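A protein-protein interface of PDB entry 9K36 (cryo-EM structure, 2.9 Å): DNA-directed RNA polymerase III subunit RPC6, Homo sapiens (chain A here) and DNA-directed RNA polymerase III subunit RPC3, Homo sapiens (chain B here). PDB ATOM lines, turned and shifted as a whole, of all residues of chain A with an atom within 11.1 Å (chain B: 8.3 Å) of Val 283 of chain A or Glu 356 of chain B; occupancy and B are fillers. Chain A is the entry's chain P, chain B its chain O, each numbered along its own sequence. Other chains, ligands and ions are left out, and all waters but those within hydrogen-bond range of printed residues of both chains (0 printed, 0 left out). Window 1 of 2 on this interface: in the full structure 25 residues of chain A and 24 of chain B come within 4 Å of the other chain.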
ATOM      1  N   ASP A 245      33.140  34.957 -28.902  1.00  0.00           N
ATOM      2  CA  ASP A 245      33.183  34.128 -27.705  1.00  0.00           C
ATOM      3  C   ASP A 245      32.507  34.786 -26.508  1.00  0.00           C
ATOM      4  O   ASP A 245      32.402  34.154 -25.452  1.00  0.00           O
ATOM      5  CB  ASP A 245      34.634  33.782 -27.359  1.00  0.00           C
ATOM      6  CG  ASP A 245      34.757  32.499 -26.560  1.00  0.00           C
ATOM      7  OD1 ASP A 245      33.722  31.835 -26.332  1.00  0.00           O
ATOM      8  OD2 ASP A 245      35.888  32.149 -26.163  1.00  0.00           O
ATOM      9  N   PRO A 275      31.190  39.025 -18.531  1.00  0.00           N
ATOM     10  CA  PRO A 275      29.896  38.572 -19.052  1.00  0.00           C
ATOM     11  C   PRO A 275      28.735  39.280 -18.374  1.00  0.00           C
ATOM     12  O   PRO A 275      28.864  39.835 -17.279  1.00  0.00           O
ATOM     13  CB  PRO A 275      29.892  37.070 -18.742  1.00  0.00           C
ATOM     14  CG  PRO A 275      30.881  36.905 -17.635  1.00  0.00           C
ATOM     15  CD  PRO A 275      31.940  37.928 -17.894  1.00  0.00           C
ATOM     16  N   ILE A 277      25.632  38.032 -17.275  1.00  0.00           N
ATOM     17  CA  ILE A 277      25.089  37.333 -16.113  1.00  0.00           C
ATOM     18  C   ILE A 277      25.870  36.047 -15.892  1.00  0.00           C
ATOM     19  O   ILE A 277      26.430  35.467 -16.833  1.00  0.00           O
ATOM     20  CB  ILE A 277      23.589  37.016 -16.280  1.00  0.00           C
ATOM     21  CG1 ILE A 277      23.351  36.203 -17.555  1.00  0.00           C
ATOM     22  CG2 ILE A 277      22.767  38.297 -16.295  1.00  0.00           C
ATOM     23  CD1 ILE A 277      21.904  35.825 -17.778  1.00  0.00           C
ATOM     24  N   PRO A 278      25.933  35.583 -14.645  1.00  0.00           N
ATOM     25  CA  PRO A 278      26.566  34.291 -14.359  1.00  0.00           C
ATOM     26  C   PRO A 278      25.797  33.155 -15.013  1.00  0.00           C
ATOM     27  O   PRO A 278      24.696  33.371 -15.546  1.00  0.00           O
ATOM     28  CB  PRO A 278      26.500  34.200 -12.825  1.00  0.00           C
ATOM     29  CG  PRO A 278      26.394  35.613 -12.369  1.00  0.00           C
ATOM     30  CD  PRO A 278      25.571  36.304 -13.414  1.00  0.00           C
ATOM     31  N   PRO A 279      26.345  31.937 -15.015  1.00  0.00           N
ATOM     32  CA  PRO A 279      25.603  30.800 -15.575  1.00  0.00           C
ATOM     33  C   PRO A 279      24.234  30.649 -14.929  1.00  0.00           C
ATOM     34  O   PRO A 279      24.080  30.770 -13.712  1.00  0.00           O
ATOM     35  CB  PRO A 279      26.511  29.605 -15.265  1.00  0.00           C
ATOM     36  CG  PRO A 279      27.879  30.189 -15.244  1.00  0.00           C
ATOM     37  CD  PRO A 279      27.729  31.569 -14.659  1.00  0.00           C
ATOM     38  N   THR A 280      23.235  30.388 -15.768  1.00  0.00           N
ATOM     39  CA  THR A 280      21.854  30.336 -15.315  1.00  0.00           C
ATOM     40  C   THR A 280      21.609  29.091 -14.463  1.00  0.00           C
ATOM     41  O   THR A 280      22.432  28.176 -14.389  1.00  0.00           O
ATOM     42  CB  THR A 280      20.900  30.356 -16.509  1.00  0.00           C
ATOM     43  OG1 THR A 280      21.130  29.204 -17.330  1.00  0.00           O
ATOM     44  CG2 THR A 280      21.121  31.612 -17.337  1.00  0.00           C
ATOM     45  N   GLY A 281      20.449  29.072 -13.807  1.00  0.00           N
ATOM     46  CA  GLY A 281      20.089  27.954 -12.950  1.00  0.00           C
ATOM     47  C   GLY A 281      19.732  26.687 -13.697  1.00  0.00           C
ATOM     48  O   GLY A 281      19.819  25.599 -13.119  1.00  0.00           O
ATOM     49  N   LEU A 282      19.330  26.801 -14.966  1.00  0.00           N
ATOM     50  CA  LEU A 282      18.954  25.616 -15.731  1.00  0.00           C
ATOM     51  C   LEU A 282      20.145  24.689 -15.936  1.00  0.00           C
ATOM     52  O   LEU A 282      20.019  23.465 -15.809  1.00  0.00           O
ATOM     53  CB  LEU A 282      18.361  26.024 -17.078  1.00  0.00           C
ATOM     54  CG  LEU A 282      18.081  24.869 -18.042  1.00  0.00           C
ATOM     55  CD1 LEU A 282      16.990  23.957 -17.496  1.00  0.00           C
ATOM     56  CD2 LEU A 282      17.716  25.389 -19.424  1.00  0.00           C
ATOM     57  N   VAL A 283      21.312  25.253 -16.257  1.00  0.00           N
ATOM     58  CA  VAL A 283      22.497  24.441 -16.504  1.00  0.00           C
ATOM     59  C   VAL A 283      23.055  23.817 -15.234  1.00  0.00           C
ATOM     60  O   VAL A 283      23.897  22.916 -15.315  1.00  0.00           O
ATOM     61  CB  VAL A 283      23.593  25.278 -17.193  1.00  0.00           C
ATOM     62  CG1 VAL A 283      23.007  26.040 -18.370  1.00  0.00           C
ATOM     63  CG2 VAL A 283      24.242  26.230 -16.204  1.00  0.00           C
ATOM     64  N   ARG A 284      22.607  24.272 -14.065  1.00  0.00           N
ATOM     65  CA  ARG A 284      23.036  23.679 -12.805  1.00  0.00           C
ATOM     66  C   ARG A 284      22.274  22.407 -12.464  1.00  0.00           C
ATOM     67  O   ARG A 284      22.584  21.768 -11.452  1.00  0.00           O
ATOM     68  CB  ARG A 284      22.886  24.694 -11.669  1.00  0.00           C
ATOM     69  CG  ARG A 284      23.780  25.917 -11.818  1.00  0.00           C
ATOM     70  CD  ARG A 284      23.715  26.805 -10.587  1.00  0.00           C
ATOM     71  NE  ARG A 284      24.680  27.900 -10.646  1.00  0.00           N
ATOM     72  CZ  ARG A 284      24.416  29.103 -11.145  1.00  0.00           C
ATOM     73  NH1 ARG A 284      23.213  29.372 -11.632  1.00  0.00           N
ATOM     74  NH2 ARG A 284      25.358  30.039 -11.158  1.00  0.00           N
ATOM     75  N   ALA A 285      21.291  22.025 -13.280  1.00  0.00           N
ATOM     76  CA  ALA A 285      20.532  20.801 -13.101  1.00  0.00           C
ATOM     77  C   ALA A 285      20.854  19.816 -14.215  1.00  0.00           C
ATOM     78  O   ALA A 285      21.066  20.229 -15.362  1.00  0.00           O
ATOM     79  CB  ALA A 285      19.025  21.079 -13.088  1.00  0.00           C
ATOM     80  N   PRO A 286      20.908  18.515 -13.916  1.00  0.00           N
ATOM     81  CA  PRO A 286      21.212  17.538 -14.975  1.00  0.00           C
ATOM     82  C   PRO A 286      20.179  17.502 -16.086  1.00  0.00           C
ATOM     83  O   PRO A 286      20.512  17.115 -17.213  1.00  0.00           O
ATOM     84  CB  PRO A 286      21.270  16.204 -14.213  1.00  0.00           C
ATOM     85  CG  PRO A 286      21.531  16.584 -12.790  1.00  0.00           C
ATOM     86  CD  PRO A 286      20.811  17.884 -12.589  1.00  0.00           C
ATOM     87  N   CYS A 287      18.933  17.891 -15.803  1.00  0.00           N
ATOM     88  CA  CYS A 287      17.892  17.848 -16.823  1.00  0.00           C
ATOM     89  C   CYS A 287      18.147  18.862 -17.931  1.00  0.00           C
ATOM     90  O   CYS A 287      17.764  18.633 -19.083  1.00  0.00           O
ATOM     91  CB  CYS A 287      16.523  18.099 -16.192  1.00  0.00           C
ATOM     92  SG  CYS A 287      16.282  17.329 -14.574  1.00  0.00           S
ATOM     93  N   GLY A 288      18.790  19.986 -17.605  1.00  0.00           N
ATOM     94  CA  GLY A 288      19.052  21.014 -18.594  1.00  0.00           C
ATOM     95  C   GLY A 288      20.169  20.681 -19.558  1.00  0.00           C
ATOM     96  O   GLY A 288      20.201  21.228 -20.665  1.00  0.00           O
ATOM     97  N   LEU A 289      21.086  19.797 -19.168  1.00  0.00           N
ATOM     98  CA  LEU A 289      22.198  19.400 -20.021  1.00  0.00           C
ATOM     99  C   LEU A 289      22.064  17.969 -20.528  1.00  0.00           C
ATOM    100  O   LEU A 289      23.039  17.409 -21.039  1.00  0.00           O
ATOM    101  CB  LEU A 289      23.524  19.568 -19.274  1.00  0.00           C
ATOM    102  CG  LEU A 289      23.758  20.934 -18.625  1.00  0.00           C
ATOM    103  CD1 LEU A 289      25.119  20.983 -17.952  1.00  0.00           C
ATOM    104  CD2 LEU A 289      23.618  22.047 -19.649  1.00  0.00           C
ATOM    105  N   CYS A 290      20.887  17.373 -20.402  1.00  0.00           N
ATOM    106  CA  CYS A 290      20.708  15.984 -20.811  1.00  0.00           C
ATOM    107  C   CYS A 290      20.615  15.885 -22.329  1.00  0.00           C
ATOM    108  O   CYS A 290      19.897  16.676 -22.955  1.00  0.00           O
ATOM    109  CB  CYS A 290      19.452  15.405 -20.167  1.00  0.00           C
ATOM    110  SG  CYS A 290      19.105  13.697 -20.631  1.00  0.00           S
ATOM    111  N   PRO A 291      21.317  14.937 -22.958  1.00  0.00           N
ATOM    112  CA  PRO A 291      21.183  14.771 -24.414  1.00  0.00           C
ATOM    113  C   PRO A 291      19.983  13.937 -24.830  1.00  0.00           C
ATOM    114  O   PRO A 291      19.601  13.985 -26.008  1.00  0.00           O
ATOM    115  CB  PRO A 291      22.494  14.074 -24.804  1.00  0.00           C
ATOM    116  CG  PRO A 291      22.838  13.268 -23.596  1.00  0.00           C
ATOM    117  CD  PRO A 291      22.362  14.063 -22.396  1.00  0.00           C
ATOM    118  N   TYR A 309      22.164  10.286 -14.509  1.00  0.00           N
ATOM    119  CA  TYR A 309      22.740  11.626 -14.441  1.00  0.00           C
ATOM    120  C   TYR A 309      22.513  12.253 -13.071  1.00  0.00           C
ATOM    121  O   TYR A 309      23.458  12.717 -12.423  1.00  0.00           O
ATOM    122  CB  TYR A 309      22.145  12.513 -15.536  1.00  0.00           C
ATOM    123  CG  TYR A 309      22.360  12.005 -16.941  1.00  0.00           C
ATOM    124  CD1 TYR A 309      23.537  12.279 -17.625  1.00  0.00           C
ATOM    125  CD2 TYR A 309      21.382  11.262 -17.591  1.00  0.00           C
ATOM    126  CE1 TYR A 309      23.740  11.822 -18.912  1.00  0.00           C
ATOM    127  CE2 TYR A 309      21.577  10.801 -18.881  1.00  0.00           C
ATOM    128  CZ  TYR A 309      22.757  11.085 -19.535  1.00  0.00           C
ATOM    129  OH  TYR A 309      22.960  10.630 -20.816  1.00  0.00           O
ATOM    130  N   MET A 310      21.257  12.279 -12.616  1.00  0.00           N
ATOM    131  CA  MET A 310      20.969  12.851 -11.306  1.00  0.00           C
ATOM    132  C   MET A 310      21.583  12.025 -10.183  1.00  0.00           C
ATOM    133  O   MET A 310      21.963  12.581  -9.150  1.00  0.00           O
ATOM    134  CB  MET A 310      19.459  12.992 -11.111  1.00  0.00           C
ATOM    135  CG  MET A 310      18.849  14.108 -11.941  1.00  0.00           C
ATOM    136  SD  MET A 310      17.118  14.409 -11.554  1.00  0.00           S
ATOM    137  CE  MET A 310      16.385  12.884 -12.135  1.00  0.00           C
ATOM    138  N   TRP A 313      25.111  13.092 -10.074  1.00  0.00           N
ATOM    139  CA  TRP A 313      25.160  14.490  -9.657  1.00  0.00           C
ATOM    140  C   TRP A 313      24.942  14.634  -8.156  1.00  0.00           C
ATOM    141  O   TRP A 313      25.622  15.431  -7.499  1.00  0.00           O
ATOM    142  CB  TRP A 313      24.125  15.292 -10.446  1.00  0.00           C
ATOM    143  CG  TRP A 313      23.914  16.692  -9.965  1.00  0.00           C
ATOM    144  CD1 TRP A 313      24.825  17.707  -9.962  1.00  0.00           C
ATOM    145  CD2 TRP A 313      22.701  17.239  -9.439  1.00  0.00           C
ATOM    146  NE1 TRP A 313      24.257  18.848  -9.453  1.00  0.00           N
ATOM    147  CE2 TRP A 313      22.952  18.588  -9.126  1.00  0.00           C
ATOM    148  CE3 TRP A 313      21.426  16.715  -9.198  1.00  0.00           C
ATOM    149  CZ2 TRP A 313      21.976  19.422  -8.586  1.00  0.00           C
ATOM    150  CZ3 TRP A 313      20.462  17.541  -8.661  1.00  0.00           C
ATOM    151  CH2 TRP A 313      20.741  18.879  -8.360  1.00  0.00           C
ATOM    152  N   THR B 349      20.039  35.270 -21.772  1.00  0.00           N
ATOM    153  CA  THR B 349      19.637  33.970 -21.240  1.00  0.00           C
ATOM    154  C   THR B 349      19.818  32.868 -22.279  1.00  0.00           C
ATOM    155  O   THR B 349      20.325  31.782 -21.969  1.00  0.00           O
ATOM    156  CB  THR B 349      18.184  34.028 -20.766  1.00  0.00           C
ATOM    157  OG1 THR B 349      18.095  34.846 -19.592  1.00  0.00           O
ATOM    158  CG2 THR B 349      17.657  32.633 -20.457  1.00  0.00           C
ATOM    159  N   LEU B 350      19.418  33.137 -23.524  1.00  0.00           N
ATOM    160  CA  LEU B 350      19.521  32.123 -24.568  1.00  0.00           C
ATOM    161  C   LEU B 350      20.977  31.805 -24.892  1.00  0.00           C
ATOM    162  O   LEU B 350      21.348  30.633 -25.028  1.00  0.00           O
ATOM    163  CB  LEU B 350      18.773  32.584 -25.818  1.00  0.00           C
ATOM    164  CG  LEU B 350      18.526  31.532 -26.899  1.00  0.00           C
ATOM    165  CD1 LEU B 350      17.870  30.295 -26.303  1.00  0.00           C
ATOM    166  CD2 LEU B 350      17.666  32.111 -28.010  1.00  0.00           C
ATOM    167  N   GLU B 351      21.823  32.832 -25.009  1.00  0.00           N
ATOM    168  CA  GLU B 351      23.228  32.571 -25.295  1.00  0.00           C
ATOM    169  C   GLU B 351      23.901  31.861 -24.125  1.00  0.00           C
ATOM    170  O   GLU B 351      24.770  31.005 -24.330  1.00  0.00           O
ATOM    171  CB  GLU B 351      23.958  33.870 -25.646  1.00  0.00           C
ATOM    172  CG  GLU B 351      24.134  34.846 -24.498  1.00  0.00           C
ATOM    173  CD  GLU B 351      24.852  36.114 -24.915  1.00  0.00           C
ATOM    174  OE1 GLU B 351      25.081  36.297 -26.129  1.00  0.00           O
ATOM    175  OE2 GLU B 351      25.187  36.931 -24.030  1.00  0.00           O
ATOM    176  N   SER B 352      23.484  32.166 -22.893  1.00  0.00           N
ATOM    177  CA  SER B 352      24.057  31.494 -21.734  1.00  0.00           C
ATOM    178  C   SER B 352      23.669  30.022 -21.697  1.00  0.00           C
ATOM    179  O   SER B 352      24.510  29.159 -21.415  1.00  0.00           O
ATOM    180  CB  SER B 352      23.620  32.198 -20.451  1.00  0.00           C
ATOM    181  OG  SER B 352      24.158  31.554 -19.308  1.00  0.00           O
ATOM    182  N   VAL B 353      22.401  29.708 -21.981  1.00  0.00           N
ATOM    183  CA  VAL B 353      21.988  28.309 -21.959  1.00  0.00           C
ATOM    184  C   VAL B 353      22.629  27.546 -23.113  1.00  0.00           C
ATOM    185  O   VAL B 353      23.014  26.379 -22.962  1.00  0.00           O
ATOM    186  CB  VAL B 353      20.450  28.182 -21.954  1.00  0.00           C
ATOM    187  CG1 VAL B 353      19.840  28.698 -23.242  1.00  0.00           C
ATOM    188  CG2 VAL B 353      20.037  26.736 -21.714  1.00  0.00           C
ATOM    189  N   VAL B 354      22.803  28.199 -24.269  1.00  0.00           N
ATOM    190  CA  VAL B 354      23.502  27.554 -25.379  1.00  0.00           C
ATOM    191  C   VAL B 354      24.953  27.270 -25.002  1.00  0.00           C
ATOM    192  O   VAL B 354      25.475  26.180 -25.272  1.00  0.00           O
ATOM    193  CB  VAL B 354      23.403  28.422 -26.648  1.00  0.00           C
ATOM    194  CG1 VAL B 354      24.389  27.942 -27.703  1.00  0.00           C
ATOM    195  CG2 VAL B 354      21.985  28.390 -27.197  1.00  0.00           C
ATOM    196  N   GLN B 355      25.621  28.238 -24.368  1.00  0.00           N
ATOM    197  CA  GLN B 355      27.009  28.044 -23.965  1.00  0.00           C
ATOM    198  C   GLN B 355      27.139  26.918 -22.946  1.00  0.00           C
ATOM    199  O   GLN B 355      28.056  26.094 -23.033  1.00  0.00           O
ATOM    200  CB  GLN B 355      27.576  29.345 -23.396  1.00  0.00           C
ATOM    201  CG  GLN B 355      29.040  29.262 -22.995  1.00  0.00           C
ATOM    202  CD  GLN B 355      29.579  30.582 -22.479  1.00  0.00           C
ATOM    203  OE1 GLN B 355      28.887  31.598 -22.496  1.00  0.00           O
ATOM    204  NE2 GLN B 355      30.824  30.571 -22.016  1.00  0.00           N
ATOM    205  N   GLU B 356      26.230  26.867 -21.970  1.00  0.00           N
ATOM    206  CA  GLU B 356      26.320  25.846 -20.936  1.00  0.00           C
ATOM    207  C   GLU B 356      25.847  24.480 -21.417  1.00  0.00           C
ATOM    208  O   GLU B 356      26.167  23.471 -20.776  1.00  0.00           O
ATOM    209  CB  GLU B 356      25.520  26.273 -19.704  1.00  0.00           C
ATOM    210  CG  GLU B 356      26.101  27.471 -18.968  1.00  0.00           C
ATOM    211  CD  GLU B 356      27.433  27.168 -18.304  1.00  0.00           C
ATOM    212  OE1 GLU B 356      27.721  25.978 -18.053  1.00  0.00           O
ATOM    213  OE2 GLU B 356      28.195  28.118 -18.035  1.00  0.00           O
ATOM    214  N   ARG B 357      25.103  24.412 -22.520  1.00  0.00           N
ATOM    215  CA  ARG B 357      24.648  23.123 -23.020  1.00  0.00           C
ATOM    216  C   ARG B 357      25.556  22.543 -24.099  1.00  0.00           C
ATOM    217  O   ARG B 357      25.677  21.317 -24.196  1.00  0.00           O
ATOM    218  CB  ARG B 357      23.219  23.241 -23.560  1.00  0.00           C
ATOM    219  CG  ARG B 357      22.579  21.909 -23.918  1.00  0.00           C
ATOM    220  CD  ARG B 357      21.143  22.084 -24.382  1.00  0.00           C
ATOM    221  NE  ARG B 357      20.544  20.812 -24.777  1.00  0.00           N
ATOM    222  CZ  ARG B 357      19.316  20.685 -25.265  1.00  0.00           C
ATOM    223  NH1 ARG B 357      18.549  21.754 -25.424  1.00  0.00           N
ATOM    224  NH2 ARG B 357      18.852  19.487 -25.598  1.00  0.00           N
ATOM    225  N   PHE B 358      26.204  23.385 -24.908  1.00  0.00           N
ATOM    226  CA  PHE B 358      27.012  22.889 -26.013  1.00  0.00           C
ATOM    227  C   PHE B 358      28.433  23.438 -26.051  1.00  0.00           C
ATOM    228  O   PHE B 358      29.172  23.113 -26.988  1.00  0.00           O
ATOM    229  CB  PHE B 358      26.325  23.189 -27.354  1.00  0.00           C
ATOM    230  CG  PHE B 358      24.960  22.581 -27.488  1.00  0.00           C
ATOM    231  CD1 PHE B 358      24.813  21.226 -27.733  1.00  0.00           C
ATOM    232  CD2 PHE B 358      23.826  23.365 -27.377  1.00  0.00           C
ATOM    233  CE1 PHE B 358      23.557  20.662 -27.859  1.00  0.00           C
ATOM    234  CE2 PHE B 358      22.567  22.808 -27.505  1.00  0.00           C
ATOM    235  CZ  PHE B 358      22.435  21.455 -27.745  1.00  0.00           C
ATOM    236  N   GLY B 359      28.836  24.254 -25.084  1.00  0.00           N
ATOM    237  CA  GLY B 359      30.192  24.758 -25.029  1.00  0.00           C
ATOM    238  C   GLY B 359      30.308  26.191 -25.524  1.00  0.00           C
ATOM    239  O   GLY B 359      29.341  26.821 -25.961  1.00  0.00           O
ATOM    240  N   SER B 360      31.537  26.707 -25.446  1.00  0.00           N
ATOM    241  CA  SER B 360      31.788  28.100 -25.811  1.00  0.00           C
ATOM    242  C   SER B 360      31.830  28.298 -27.320  1.00  0.00           C
ATOM    243  O   SER B 360      31.440  29.362 -27.811  1.00  0.00           O
ATOM    244  CB  SER B 360      33.095  28.579 -25.177  1.00  0.00           C
ATOM    245  OG  SER B 360      33.040  28.496 -23.765  1.00  0.00           O
ATOM    246  N   CYS B 362      30.062  26.635 -29.623  1.00  0.00           N
ATOM    247  CA  CYS B 362      28.683  26.676 -30.094  1.00  0.00           C
ATOM    248  C   CYS B 362      28.024  28.001 -29.735  1.00  0.00           C
ATOM    249  O   CYS B 362      27.216  28.527 -30.507  1.00  0.00           O
ATOM    250  CB  CYS B 362      27.894  25.504 -29.514  1.00  0.00           C
ATOM    251  SG  CYS B 362      26.207  25.370 -30.145  1.00  0.00           S
ATOM    252  N   ALA B 363      28.368  28.563 -28.575  1.00  0.00           N
ATOM    253  CA  ALA B 363      27.862  29.884 -28.222  1.00  0.00           C
ATOM    254  C   ALA B 363      28.412  30.951 -29.161  1.00  0.00           C
ATOM    255  O   ALA B 363      27.706  31.905 -29.512  1.00  0.00           O
ATOM    256  CB  ALA B 363      28.218  30.216 -26.773  1.00  0.00           C
ATOM    257  N   ARG B 367      26.050  33.348 -31.403  1.00  0.00           N
ATOM    258  CA  ARG B 367      26.094  34.806 -31.436  1.00  0.00           C
ATOM    259  C   ARG B 367      26.414  35.315 -32.837  1.00  0.00           C
ATOM    260  O   ARG B 367      25.923  36.376 -33.244  1.00  0.00           O
ATOM    261  CB  ARG B 367      27.109  35.327 -30.422  1.00  0.00           C
ATOM    262  CG  ARG B 367      26.771  34.989 -28.978  1.00  0.00           C
ATOM    263  CD  ARG B 367      27.727  35.664 -28.012  1.00  0.00           C
ATOM    264  NE  ARG B 367      27.489  35.262 -26.629  1.00  0.00           N
ATOM    265  CZ  ARG B 367      28.097  34.239 -26.035  1.00  0.00           C
ATOM    266  NH1 ARG B 367      28.983  33.513 -26.702  1.00  0.00           N
ATOM    267  NH2 ARG B 367      27.819  33.944 -24.772  1.00  0.00           N
ATOM    268  N   CYS B 439      11.940  24.720 -19.419  1.00  0.00           N
ATOM    269  CA  CYS B 439      12.052  25.039 -17.999  1.00  0.00           C
ATOM    270  C   CYS B 439      10.849  24.520 -17.219  1.00  0.00           C
ATOM    271  O   CYS B 439      10.992  24.030 -16.092  1.00  0.00           O
ATOM    272  CB  CYS B 439      12.200  26.549 -17.808  1.00  0.00           C
ATOM    273  SG  CYS B 439      13.732  27.256 -18.453  1.00  0.00           S
ATOM    274  N   SER B 442      11.349  20.896 -16.841  1.00  0.00           N
ATOM    275  CA  SER B 442      12.452  20.663 -15.914  1.00  0.00           C
ATOM    276  C   SER B 442      11.987  20.791 -14.469  1.00  0.00           C
ATOM    277  O   SER B 442      12.314  19.949 -13.621  1.00  0.00           O
ATOM    278  CB  SER B 442      13.588  21.644 -16.202  1.00  0.00           C
ATOM    279  OG  SER B 442      14.608  21.546 -15.223  1.00  0.00           O
ATOM    280  N   SER B 512      17.280  24.323  -6.822  1.00  0.00           N
ATOM    281  CA  SER B 512      17.264  24.367  -8.282  1.00  0.00           C
ATOM    282  C   SER B 512      15.885  24.753  -8.810  1.00  0.00           C
ATOM    283  O   SER B 512      15.776  25.523  -9.771  1.00  0.00           O
ATOM    284  CB  SER B 512      17.702  23.021  -8.854  1.00  0.00           C
ATOM    285  OG  SER B 512      19.031  22.722  -8.475  1.00  0.00           O
ATOM    286  N   VAL B 516      15.419  28.071 -11.157  1.00  0.00           N
ATOM    287  CA  VAL B 516      14.893  28.017 -12.521  1.00  0.00           C
ATOM    288  C   VAL B 516      13.726  28.986 -12.679  1.00  0.00           C
ATOM    289  O   VAL B 516      13.428  29.444 -13.792  1.00  0.00           O
ATOM    290  CB  VAL B 516      14.500  26.569 -12.881  1.00  0.00           C
ATOM    291  CG1 VAL B 516      13.820  26.503 -14.243  1.00  0.00           C
ATOM    292  CG2 VAL B 516      15.727  25.676 -12.879  1.00  0.00           C
ATOM    293  N   THR B 519      14.707  32.260 -14.513  1.00  0.00           N
ATOM    294  CA  THR B 519      14.709  32.138 -15.967  1.00  0.00           C
ATOM    295  C   THR B 519      13.287  32.050 -16.504  1.00  0.00           C
ATOM    296  O   THR B 519      12.978  32.609 -17.565  1.00  0.00           O
ATOM    297  CB  THR B 519      15.521  30.914 -16.391  1.00  0.00           C
ATOM    298  OG1 THR B 519      16.828  30.982 -15.808  1.00  0.00           O
ATOM    299  CG2 THR B 519      15.649  30.855 -17.905  1.00  0.00           C
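Printed residues of chain A that touch a printed residue of chain B: Asp 245, Pro 279, Thr 280, Leu 282, Val 283, Gly 288, Leu 289 and Cys 290. Hydrophobic or aromatic side chains of chain A that line the printed part of chain B: Pro 279, Leu 282, Val 283 and Leu 289. Printed residues of chain B that touch a printed residue of chain A: Ser 352, Val 353, Glu 356, Arg 357, Ser 360 and Arg 367. Among the printed residues, 10 pairs touch across the chains. Among the printed residues, no Asp or Glu carboxylate lies within 4 Å of a Lys or Arg side-chain nitrogen of the other chain.
Among the printed residues, pairs that only touch across the chains: Val 283 of chain A with Glu 356 of chain B (2.9 Å), Leu 289 of chain A with Glu 356 of chain B (3.1 Å), Pro 279 of chain A with Glu 356 of chain B (3.5 Å), Asp 245 of chain A with Ser 360 of chain B (3.5 Å), Leu 282 of chain A with Val 353 of chain B (3.5 Å), Thr 280 of chain A with Ser 352 of chain B (3.6 Å), Leu 289 of chain A with Arg 357 of chain B (3.7 Å), Asp 245 of chain A with Arg 367 of chain B (3.7 Å), Gly 288 of chain A with Arg 357 of chain B (3.9 Å) and Cys 290 of chain A with Arg 357 of chain B (3.997 Å).
NH1 of Arg 367 of chain B sits close to O of Ala 363 of chain B. The guanidinium group (NH1) of Arg 284 of chain A lies within hydrogen-bond range of the backbone carbonyl oxygen (O) of Pro 279 of chain A (2.7 Å). The side-chain carboxylate (OE1) of Glu 351 of chain B is in salt-bridge range of the guanidinium group (NE) of Arg 367 of chain B, at 2.7 Å. The backbone carbonyl oxygen of Thr 280 of chain A sits at hydrogen-bond distance from the guanidinium group of Arg 284 of chain A, at 3.1 Å. OE1 of Gln 355 of chain B sits at hydrogen-bond distance from NH2 of Arg 367 of chain B.
Of the printed residues of chain B, Thr 280 of chain A touches Ser 352. Val 283 of chain A touches one residue of chain B. Val 354 of chain B touches none of the printed residues of chain A. No residue of chain A comes within 4 Å of Gln 355 of chain B. Glu 356 of chain B touches three residues of chain A. Of the printed residues of chain A, Arg 357 of chain B touches Gly 288, Leu 289 and Cys 290. Gly 359 of chain B touches none of the printed residues of chain A. Of the printed residues of chain A, Arg 367 of chain B touches Asp 245 (3.7 Å). The nearest printed residue of chain A that does not touch Arg 357 of chain B is Val 283 of chain A (4.9 Å).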
